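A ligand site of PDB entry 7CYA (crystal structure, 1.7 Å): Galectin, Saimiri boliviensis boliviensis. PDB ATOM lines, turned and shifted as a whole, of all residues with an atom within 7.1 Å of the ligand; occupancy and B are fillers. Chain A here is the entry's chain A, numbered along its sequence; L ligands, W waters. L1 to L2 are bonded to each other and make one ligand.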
ATOM      1  N   GLN A  38      20.526  17.323 -29.875  1.00  0.00           N
ATOM      2  CA  GLN A  38      20.895  18.127 -28.728  1.00  0.00           C
ATOM      3  C   GLN A  38      19.806  19.152 -28.424  1.00  0.00           C
ATOM      4  O   GLN A  38      18.956  19.465 -29.262  1.00  0.00           O
ATOM      5  CB  GLN A  38      22.218  18.879 -28.950  1.00  0.00           C
ATOM      6  CG  GLN A  38      23.426  17.989 -29.184  1.00  0.00           C
ATOM      7  CD  GLN A  38      24.674  18.795 -29.525  1.00  0.00           C
ATOM      8  OE1 GLN A  38      24.903  19.864 -28.960  1.00  0.00           O
ATOM      9  NE2 GLN A  38      25.479  18.287 -30.442  1.00  0.00           N
ATOM     10  N   GLN A  40      19.806  23.006 -26.153  1.00  0.00           N
ATOM     11  CA  GLN A  40      20.618  23.967 -25.405  1.00  0.00           C
ATOM     12  C   GLN A  40      19.738  25.084 -24.867  1.00  0.00           C
ATOM     13  O   GLN A  40      18.895  25.621 -25.583  1.00  0.00           O
ATOM     14  CB  GLN A  40      21.763  24.525 -26.280  1.00  0.00           C
ATOM     15  CG  GLN A  40      22.775  25.417 -25.531  1.00  0.00           C
ATOM     16  CD  GLN A  40      24.145  25.492 -26.217  1.00  0.00           C
ATOM     17  OE1 GLN A  40      24.655  24.494 -26.740  1.00  0.00           O
ATOM     18  NE2 GLN A  40      24.745  26.683 -26.212  1.00  0.00           N
ATOM     19  N   HIS A  56      24.347  27.837 -18.641  1.00  0.00           N
ATOM     20  CA  HIS A  56      24.317  27.133 -19.921  1.00  0.00           C
ATOM     21  C   HIS A  56      23.984  25.678 -19.624  1.00  0.00           C
ATOM     22  O   HIS A  56      24.664  25.040 -18.822  1.00  0.00           O
ATOM     23  CB  HIS A  56      25.686  27.286 -20.596  1.00  0.00           C
ATOM     24  CG  HIS A  56      26.016  26.243 -21.626  1.00  0.00           C
ATOM     25  ND1 HIS A  56      25.609  26.337 -22.939  1.00  0.00           N
ATOM     26  CD2 HIS A  56      26.803  25.148 -21.552  1.00  0.00           C
ATOM     27  CE1 HIS A  56      26.093  25.317 -23.619  1.00  0.00           C
ATOM     28  NE2 HIS A  56      26.828  24.587 -22.811  1.00  0.00           N
ATOM     29  N   ARG A  58      23.080  22.118 -21.569  1.00  0.00           N
ATOM     30  CA  ARG A  58      23.206  21.504 -22.885  1.00  0.00           C
ATOM     31  C   ARG A  58      23.012  20.001 -22.770  1.00  0.00           C
ATOM     32  O   ARG A  58      23.798  19.318 -22.112  1.00  0.00           O
ATOM     33  CB  ARG A  58      24.564  21.820 -23.520  1.00  0.00           C
ATOM     34  CG  ARG A  58      24.690  21.357 -24.946  1.00  0.00           C
ATOM     35  CD  ARG A  58      26.034  21.789 -25.552  1.00  0.00           C
ATOM     36  NE  ARG A  58      26.190  21.391 -26.942  1.00  0.00           N
ATOM     37  CZ  ARG A  58      27.146  21.854 -27.750  1.00  0.00           C
ATOM     38  NH1 ARG A  58      28.015  22.752 -27.294  1.00  0.00           N
ATOM     39  NH2 ARG A  58      27.227  21.439 -29.005  1.00  0.00           N
ATOM     40  N   HIS A  60      23.061  16.488 -24.458  1.00  0.00           N
ATOM     41  CA  HIS A  60      23.445  15.575 -25.535  1.00  0.00           C
ATOM     42  C   HIS A  60      22.535  14.363 -25.355  1.00  0.00           C
ATOM     43  O   HIS A  60      22.842  13.439 -24.602  1.00  0.00           O
ATOM     44  CB  HIS A  60      24.927  15.227 -25.469  1.00  0.00           C
ATOM     45  CG  HIS A  60      25.834  16.411 -25.637  1.00  0.00           C
ATOM     46  ND1 HIS A  60      26.286  16.841 -26.863  1.00  0.00           N
ATOM     47  CD2 HIS A  60      26.393  17.255 -24.723  1.00  0.00           C
ATOM     48  CE1 HIS A  60      27.063  17.890 -26.709  1.00  0.00           C
ATOM     49  NE2 HIS A  60      27.156  18.162 -25.413  1.00  0.00           N
ATOM     50  N   ARG A  64      24.699  12.577 -22.275  1.00  0.00           N
ATOM     51  CA  ARG A  64      24.992  13.289 -21.034  1.00  0.00           C
ATOM     52  C   ARG A  64      24.408  14.699 -21.117  1.00  0.00           C
ATOM     53  O   ARG A  64      23.962  15.148 -22.173  1.00  0.00           O
ATOM     54  CB  ARG A  64      26.490  13.347 -20.769  1.00  0.00           C
ATOM     55  CG  ARG A  64      27.206  14.368 -21.632  1.00  0.00           C
ATOM     56  CD  ARG A  64      28.721  14.149 -21.736  1.00  0.00           C
ATOM     57  NE  ARG A  64      29.384  15.291 -22.359  1.00  0.00           N
ATOM     58  CZ  ARG A  64      29.509  15.478 -23.673  1.00  0.00           C
ATOM     59  NH1 ARG A  64      29.031  14.585 -24.526  1.00  0.00           N
ATOM     60  NH2 ARG A  64      30.119  16.569 -24.130  1.00  0.00           N
ATOM     61  N   VAL A  66      25.550  18.693 -19.855  1.00  0.00           N
ATOM     62  CA  VAL A  66      26.620  19.529 -19.337  1.00  0.00           C
ATOM     63  C   VAL A  66      26.061  20.897 -19.002  1.00  0.00           C
ATOM     64  O   VAL A  66      25.167  21.410 -19.672  1.00  0.00           O
ATOM     65  CB  VAL A  66      27.830  19.671 -20.305  1.00  0.00           C
ATOM     66  CG1 VAL A  66      28.428  18.316 -20.596  1.00  0.00           C
ATOM     67  CG2 VAL A  66      27.435  20.363 -21.593  1.00  0.00           C
ATOM     68  N   MET A  67      26.607  21.490 -17.943  1.00  0.00           N
ATOM     69  CA  MET A  67      26.218  22.823 -17.503  1.00  0.00           C
ATOM     70  C   MET A  67      27.482  23.642 -17.301  1.00  0.00           C
ATOM     71  O   MET A  67      28.541  23.102 -16.966  1.00  0.00           O
ATOM     72  CB  MET A  67      25.397  22.727 -16.213  1.00  0.00           C
ATOM     73  CG  MET A  67      24.021  22.134 -16.435  1.00  0.00           C
ATOM     74  SD  MET A  67      23.220  21.661 -14.897  1.00  0.00           S
ATOM     75  CE  MET A  67      24.175  20.186 -14.555  1.00  0.00           C
ATOM     76  N   ASN A  68      27.382  24.944 -17.513  1.00  0.00           N
ATOM     77  CA  ASN A  68      28.568  25.796 -17.410  1.00  0.00           C
ATOM     78  C   ASN A  68      28.124  27.251 -17.434  1.00  0.00           C
ATOM     79  O   ASN A  68      26.935  27.564 -17.473  1.00  0.00           O
ATOM     80  CB  ASN A  68      29.561  25.499 -18.541  1.00  0.00           C
ATOM     81  CG  ASN A  68      31.008  25.770 -18.159  1.00  0.00           C
ATOM     82  OD1 ASN A  68      31.314  26.607 -17.289  1.00  0.00           O
ATOM     83  ND2 ASN A  68      31.930  25.083 -18.831  1.00  0.00           N
ATOM     84  N   SER A  69      29.112  28.141 -17.441  1.00  0.00           N
ATOM     85  CA  SER A  69      28.895  29.554 -17.663  1.00  0.00           C
ATOM     86  C   SER A  69      29.926  30.028 -18.667  1.00  0.00           C
ATOM     87  O   SER A  69      30.982  29.412 -18.845  1.00  0.00           O
ATOM     88  CB  SER A  69      29.011  30.362 -16.366  1.00  0.00           C
ATOM     89  OG  SER A  69      30.266  30.106 -15.756  1.00  0.00           O
ATOM     90  N   TRP A  75      34.569  29.652 -21.433  1.00  0.00           N
ATOM     91  CA  TRP A  75      33.820  28.616 -20.733  1.00  0.00           C
ATOM     92  C   TRP A  75      34.511  28.287 -19.413  1.00  0.00           C
ATOM     93  O   TRP A  75      35.736  28.134 -19.370  1.00  0.00           O
ATOM     94  CB  TRP A  75      33.709  27.355 -21.591  1.00  0.00           C
ATOM     95  CG  TRP A  75      32.830  27.539 -22.772  1.00  0.00           C
ATOM     96  CD1 TRP A  75      33.204  27.570 -24.085  1.00  0.00           C
ATOM     97  CD2 TRP A  75      31.407  27.720 -22.753  1.00  0.00           C
ATOM     98  NE1 TRP A  75      32.102  27.769 -24.882  1.00  0.00           N
ATOM     99  CE2 TRP A  75      30.986  27.866 -24.086  1.00  0.00           C
ATOM    100  CE3 TRP A  75      30.460  27.785 -21.720  1.00  0.00           C
ATOM    101  CZ2 TRP A  75      29.650  28.056 -24.423  1.00  0.00           C
ATOM    102  CZ3 TRP A  75      29.140  27.977 -22.072  1.00  0.00           C
ATOM    103  CH2 TRP A  75      28.740  28.108 -23.406  1.00  0.00           C
ATOM    104  N   LYS A  76      33.743  28.185 -18.332  1.00  0.00           N
ATOM    105  CA  LYS A  76      34.345  27.972 -17.012  1.00  0.00           C
ATOM    106  C   LYS A  76      34.267  26.503 -16.641  1.00  0.00           C
ATOM    107  O   LYS A  76      34.437  25.636 -17.510  1.00  0.00           O
ATOM    108  CB  LYS A  76      33.668  28.893 -15.992  1.00  0.00           C
ATOM    109  CG  LYS A  76      33.701  30.369 -16.398  1.00  0.00           C
ATOM    110  CD  LYS A  76      35.119  30.947 -16.418  1.00  0.00           C
ATOM    111  CE  LYS A  76      35.777  30.837 -15.068  1.00  0.00           C
ATOM    112  NZ  LYS A  76      36.907  31.802 -14.948  1.00  0.00           N
ATOM    113  N   LEU A  77      34.026  26.178 -15.367  1.00  0.00           N
ATOM    114  CA  LEU A  77      34.062  24.786 -14.928  1.00  0.00           C
ATOM    115  C   LEU A  77      32.851  24.034 -15.459  1.00  0.00           C
ATOM    116  O   LEU A  77      31.706  24.405 -15.157  1.00  0.00           O
ATOM    117  CB  LEU A  77      34.108  24.692 -13.409  1.00  0.00           C
ATOM    118  CG  LEU A  77      33.918  23.274 -12.845  1.00  0.00           C
ATOM    119  CD1 LEU A  77      35.126  22.428 -13.159  1.00  0.00           C
ATOM    120  CD2 LEU A  77      33.628  23.289 -11.355  1.00  0.00           C
ATOM    121  N   GLU A  78      33.076  22.950 -16.184  1.00  0.00           N
ATOM    122  CA  GLU A  78      31.974  22.154 -16.698  1.00  0.00           C
ATOM    123  C   GLU A  78      31.459  21.213 -15.604  1.00  0.00           C
ATOM    124  O   GLU A  78      32.237  20.511 -14.957  1.00  0.00           O
ATOM    125  CB  GLU A  78      32.402  21.357 -17.934  1.00  0.00           C
ATOM    126  CG  GLU A  78      31.296  20.499 -18.528  1.00  0.00           C
ATOM    127  CD  GLU A  78      31.726  19.814 -19.811  1.00  0.00           C
ATOM    128  OE1 GLU A  78      32.236  18.669 -19.728  1.00  0.00           O
ATOM    129  OE2 GLU A  78      31.561  20.405 -20.892  1.00  0.00           O
ATOM    130  N   GLU A  79      30.140  21.211 -15.402  1.00  0.00           N
ATOM    131  CA  GLU A  79      29.452  20.302 -14.505  1.00  0.00           C
ATOM    132  C   GLU A  79      28.631  19.336 -15.357  1.00  0.00           C
ATOM    133  O   GLU A  79      27.915  19.773 -16.262  1.00  0.00           O
ATOM    134  CB  GLU A  79      28.563  21.068 -13.513  1.00  0.00           C
ATOM    135  CG  GLU A  79      29.365  22.092 -12.687  1.00  0.00           C
ATOM    136  CD  GLU A  79      28.553  22.832 -11.643  1.00  0.00           C
ATOM    137  OE1 GLU A  79      27.457  22.375 -11.276  1.00  0.00           O
ATOM    138  OE2 GLU A  79      29.036  23.896 -11.175  1.00  0.00           O
ATOM    139  N   LYS A  80      28.764  18.039 -15.121  1.00  0.00           N
ATOM    140  CA  LYS A  80      28.087  17.081 -15.975  1.00  0.00           C
ATOM    141  C   LYS A  80      27.188  16.141 -15.191  1.00  0.00           C
ATOM    142  O   LYS A  80      27.448  15.837 -14.016  1.00  0.00           O
ATOM    143  CB  LYS A  80      29.079  16.245 -16.806  1.00  0.00           C
ATOM    144  CG  LYS A  80      29.817  15.141 -16.091  1.00  0.00           C
ATOM    145  CD  LYS A  80      30.690  14.359 -17.083  1.00  0.00           C
ATOM    146  CE  LYS A  80      29.880  13.607 -18.155  1.00  0.00           C
ATOM    147  NZ  LYS A  80      29.120  12.420 -17.656  1.00  0.00           N
ATOM    148  N   TRP A 130      17.567  26.347 -28.080  1.00  0.00           N
ATOM    149  CA  TRP A 130      17.886  26.070 -29.480  1.00  0.00           C
ATOM    150  C   TRP A 130      18.456  24.663 -29.631  1.00  0.00           C
ATOM    151  O   TRP A 130      18.501  23.867 -28.677  1.00  0.00           O
ATOM    152  CB  TRP A 130      18.815  27.149 -30.038  1.00  0.00           C
ATOM    153  CG  TRP A 130      20.177  27.320 -29.380  1.00  0.00           C
ATOM    154  CD1 TRP A 130      20.423  27.692 -28.089  1.00  0.00           C
ATOM    155  CD2 TRP A 130      21.449  27.189 -30.017  1.00  0.00           C
ATOM    156  NE1 TRP A 130      21.786  27.771 -27.874  1.00  0.00           N
ATOM    157  CE2 TRP A 130      22.440  27.473 -29.041  1.00  0.00           C
ATOM    158  CE3 TRP A 130      21.856  26.845 -31.312  1.00  0.00           C
ATOM    159  CZ2 TRP A 130      23.800  27.419 -29.327  1.00  0.00           C
ATOM    160  CZ3 TRP A 130      23.208  26.794 -31.587  1.00  0.00           C
ATOM    161  CH2 TRP A 130      24.162  27.082 -30.603  1.00  0.00           C
ATOM    162  N   ARG A 131      18.889  24.369 -30.863  1.00  0.00           N
ATOM    163  CA  ARG A 131      19.359  23.069 -31.357  1.00  0.00           C
ATOM    164  C   ARG A 131      18.171  22.196 -31.751  1.00  0.00           C
ATOM    165  O   ARG A 131      17.157  22.719 -32.244  1.00  0.00           O
ATOM    166  CB  ARG A 131      20.297  22.405 -30.333  1.00  0.00           C
ATOM    167  CG  ARG A 131      21.545  23.266 -30.088  1.00  0.00           C
ATOM    168  CD  ARG A 131      22.718  22.477 -29.524  1.00  0.00           C
ATOM    169  NE  ARG A 131      23.817  23.364 -29.145  1.00  0.00           N
ATOM    170  CZ  ARG A 131      24.862  23.668 -29.928  1.00  0.00           C
ATOM    171  NH1 ARG A 131      24.967  23.172 -31.150  1.00  0.00           N
ATOM    172  NH2 ARG A 131      25.796  24.494 -29.473  1.00  0.00           N
HETATM  173  C1  LIG L   1      33.736  18.447 -23.193  1.00  0.00           C
HETATM  174  C2  LIG L   1      32.777  19.233 -23.990  1.00  0.00           C
HETATM  175  C3  LIG L   1      33.320  20.584 -24.334  1.00  0.00           C
HETATM  176  C4  LIG L   1      34.684  20.493 -25.046  1.00  0.00           C
HETATM  177  C5  LIG L   1      35.253  21.787 -25.297  1.00  0.00           C
HETATM  178  C6  LIG L   1      35.069  18.389 -23.800  1.00  0.00           C
HETATM  179  O1  LIG L   1      35.949  17.767 -22.924  1.00  0.00           O
HETATM  180  O2  LIG L   1      33.278  17.058 -23.054  1.00  0.00           O
HETATM  181  O3  LIG L   1      31.525  19.377 -23.216  1.00  0.00           O
HETATM  182  O4  LIG L   1      32.442  21.253 -25.253  1.00  0.00           O
HETATM  183  O5  LIG L   1      35.626  19.708 -24.101  1.00  0.00           O
HETATM  184  O6  LIG L   1      35.474  22.438 -24.043  1.00  0.00           O
HETATM  185  C1  LG2 L   2      32.153  22.452 -24.864  1.00  0.00           C
HETATM  186  C2  LG2 L   2      31.334  23.187 -25.976  1.00  0.00           C
HETATM  187  C3  LG2 L   2      30.725  24.467 -25.536  1.00  0.00           C
HETATM  188  C4  LG2 L   2      29.955  24.331 -24.290  1.00  0.00           C
HETATM  189  C5  LG2 L   2      30.816  23.751 -23.222  1.00  0.00           C
HETATM  190  C6  LG2 L   2      30.099  23.589 -21.897  1.00  0.00           C
HETATM  191  O1  LG2 L   2      32.256  23.425 -27.041  1.00  0.00           O
HETATM  192  O2  LG2 L   2      29.839  24.933 -26.608  1.00  0.00           O
HETATM  193  O3  LG2 L   2      28.828  23.437 -24.500  1.00  0.00           O
HETATM  194  O4  LG2 L   2      31.271  22.405 -23.620  1.00  0.00           O
HETATM  195  O5  LG2 L   2      31.041  23.185 -20.946  1.00  0.00           O
HETATM  196  O   HOH W   1      31.299  16.422 -21.002  1.00  0.00           O
HETATM  197  O   HOH W   2      31.917  21.100 -28.588  1.00  0.00           O
HETATM  198  O   HOH W   3      27.361  26.635 -27.192  1.00  0.00           O
HETATM  199  O   HOH W   4      29.311  20.412 -24.630  1.00  0.00           O
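Water W4 lies within hydrogen-bond range of O3 of LIG L1 and NE2 of His 60. Water W1 lies within hydrogen-bond range of the guanidinium group of Arg 64 (2.6 Å), the side-chain carboxylate of Glu 78 (2.7 Å) and an oxygen (O2) of LIG L1 (2.9 Å). Water W3 lies within hydrogen-bond range of the side-chain amide nitrogen (NE2) of Gln 40 (2.8 Å), an oxygen (O2) of LG2 L2 (3.1 Å) and the guanidinium group (NH2) of Arg 131 (3.5 Å).
The side-chain amide nitrogen (NE2) of Gln 40 sits close to a ring nitrogen (ND1) of His 56. O of Asn 68 lies within hydrogen-bond range of N of His 56 (2.9 Å). O of Leu 77 sits close to OD1 of Asn 68. ND2 of Asn 68 lies within hydrogen-bond range of O of Lys 76 (2.9 Å). The backbone NH (N) of Arg 58 sits at hydrogen-bond distance from the backbone carbonyl oxygen (O) of Val 66 (2.9 Å). The guanidinium group of Arg 58 lies within hydrogen-bond range of the side-chain amide oxygen of Gln 38, at 2.8 Å. NE of Arg 58 sits close to OE1 of Gln 40.
NE1 of Trp 75 touches C3 of LG2 L2, 3.6 Å away. Hydrophobic or aromatic side chains that line the ligand: His 56 and Trp 75. Of the 18 residues printed, 6 come within 4 Å of the ligand.
A ring nitrogen (NE2) of His 56 is in hydrogen-bond range of an oxygen (O3) of LG2 L2 (2.9 Å). O5 of LG2 L2 is in hydrogen-bond range of ND2 of Asn 68 (3.0 Å). An oxygen (O3) of LIG L1 sits at hydrogen-bond distance from the side-chain carboxylate (OE2) of Glu 78. The guanidinium group (NH2) of Arg 64 is in hydrogen-bond range of an oxygen (O3) of LIG L1 (3.3 Å). The guanidinium group (NH1) of Arg 58 is in hydrogen-bond range of an oxygen (O2) of LG2 L2 (2.9 Å).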
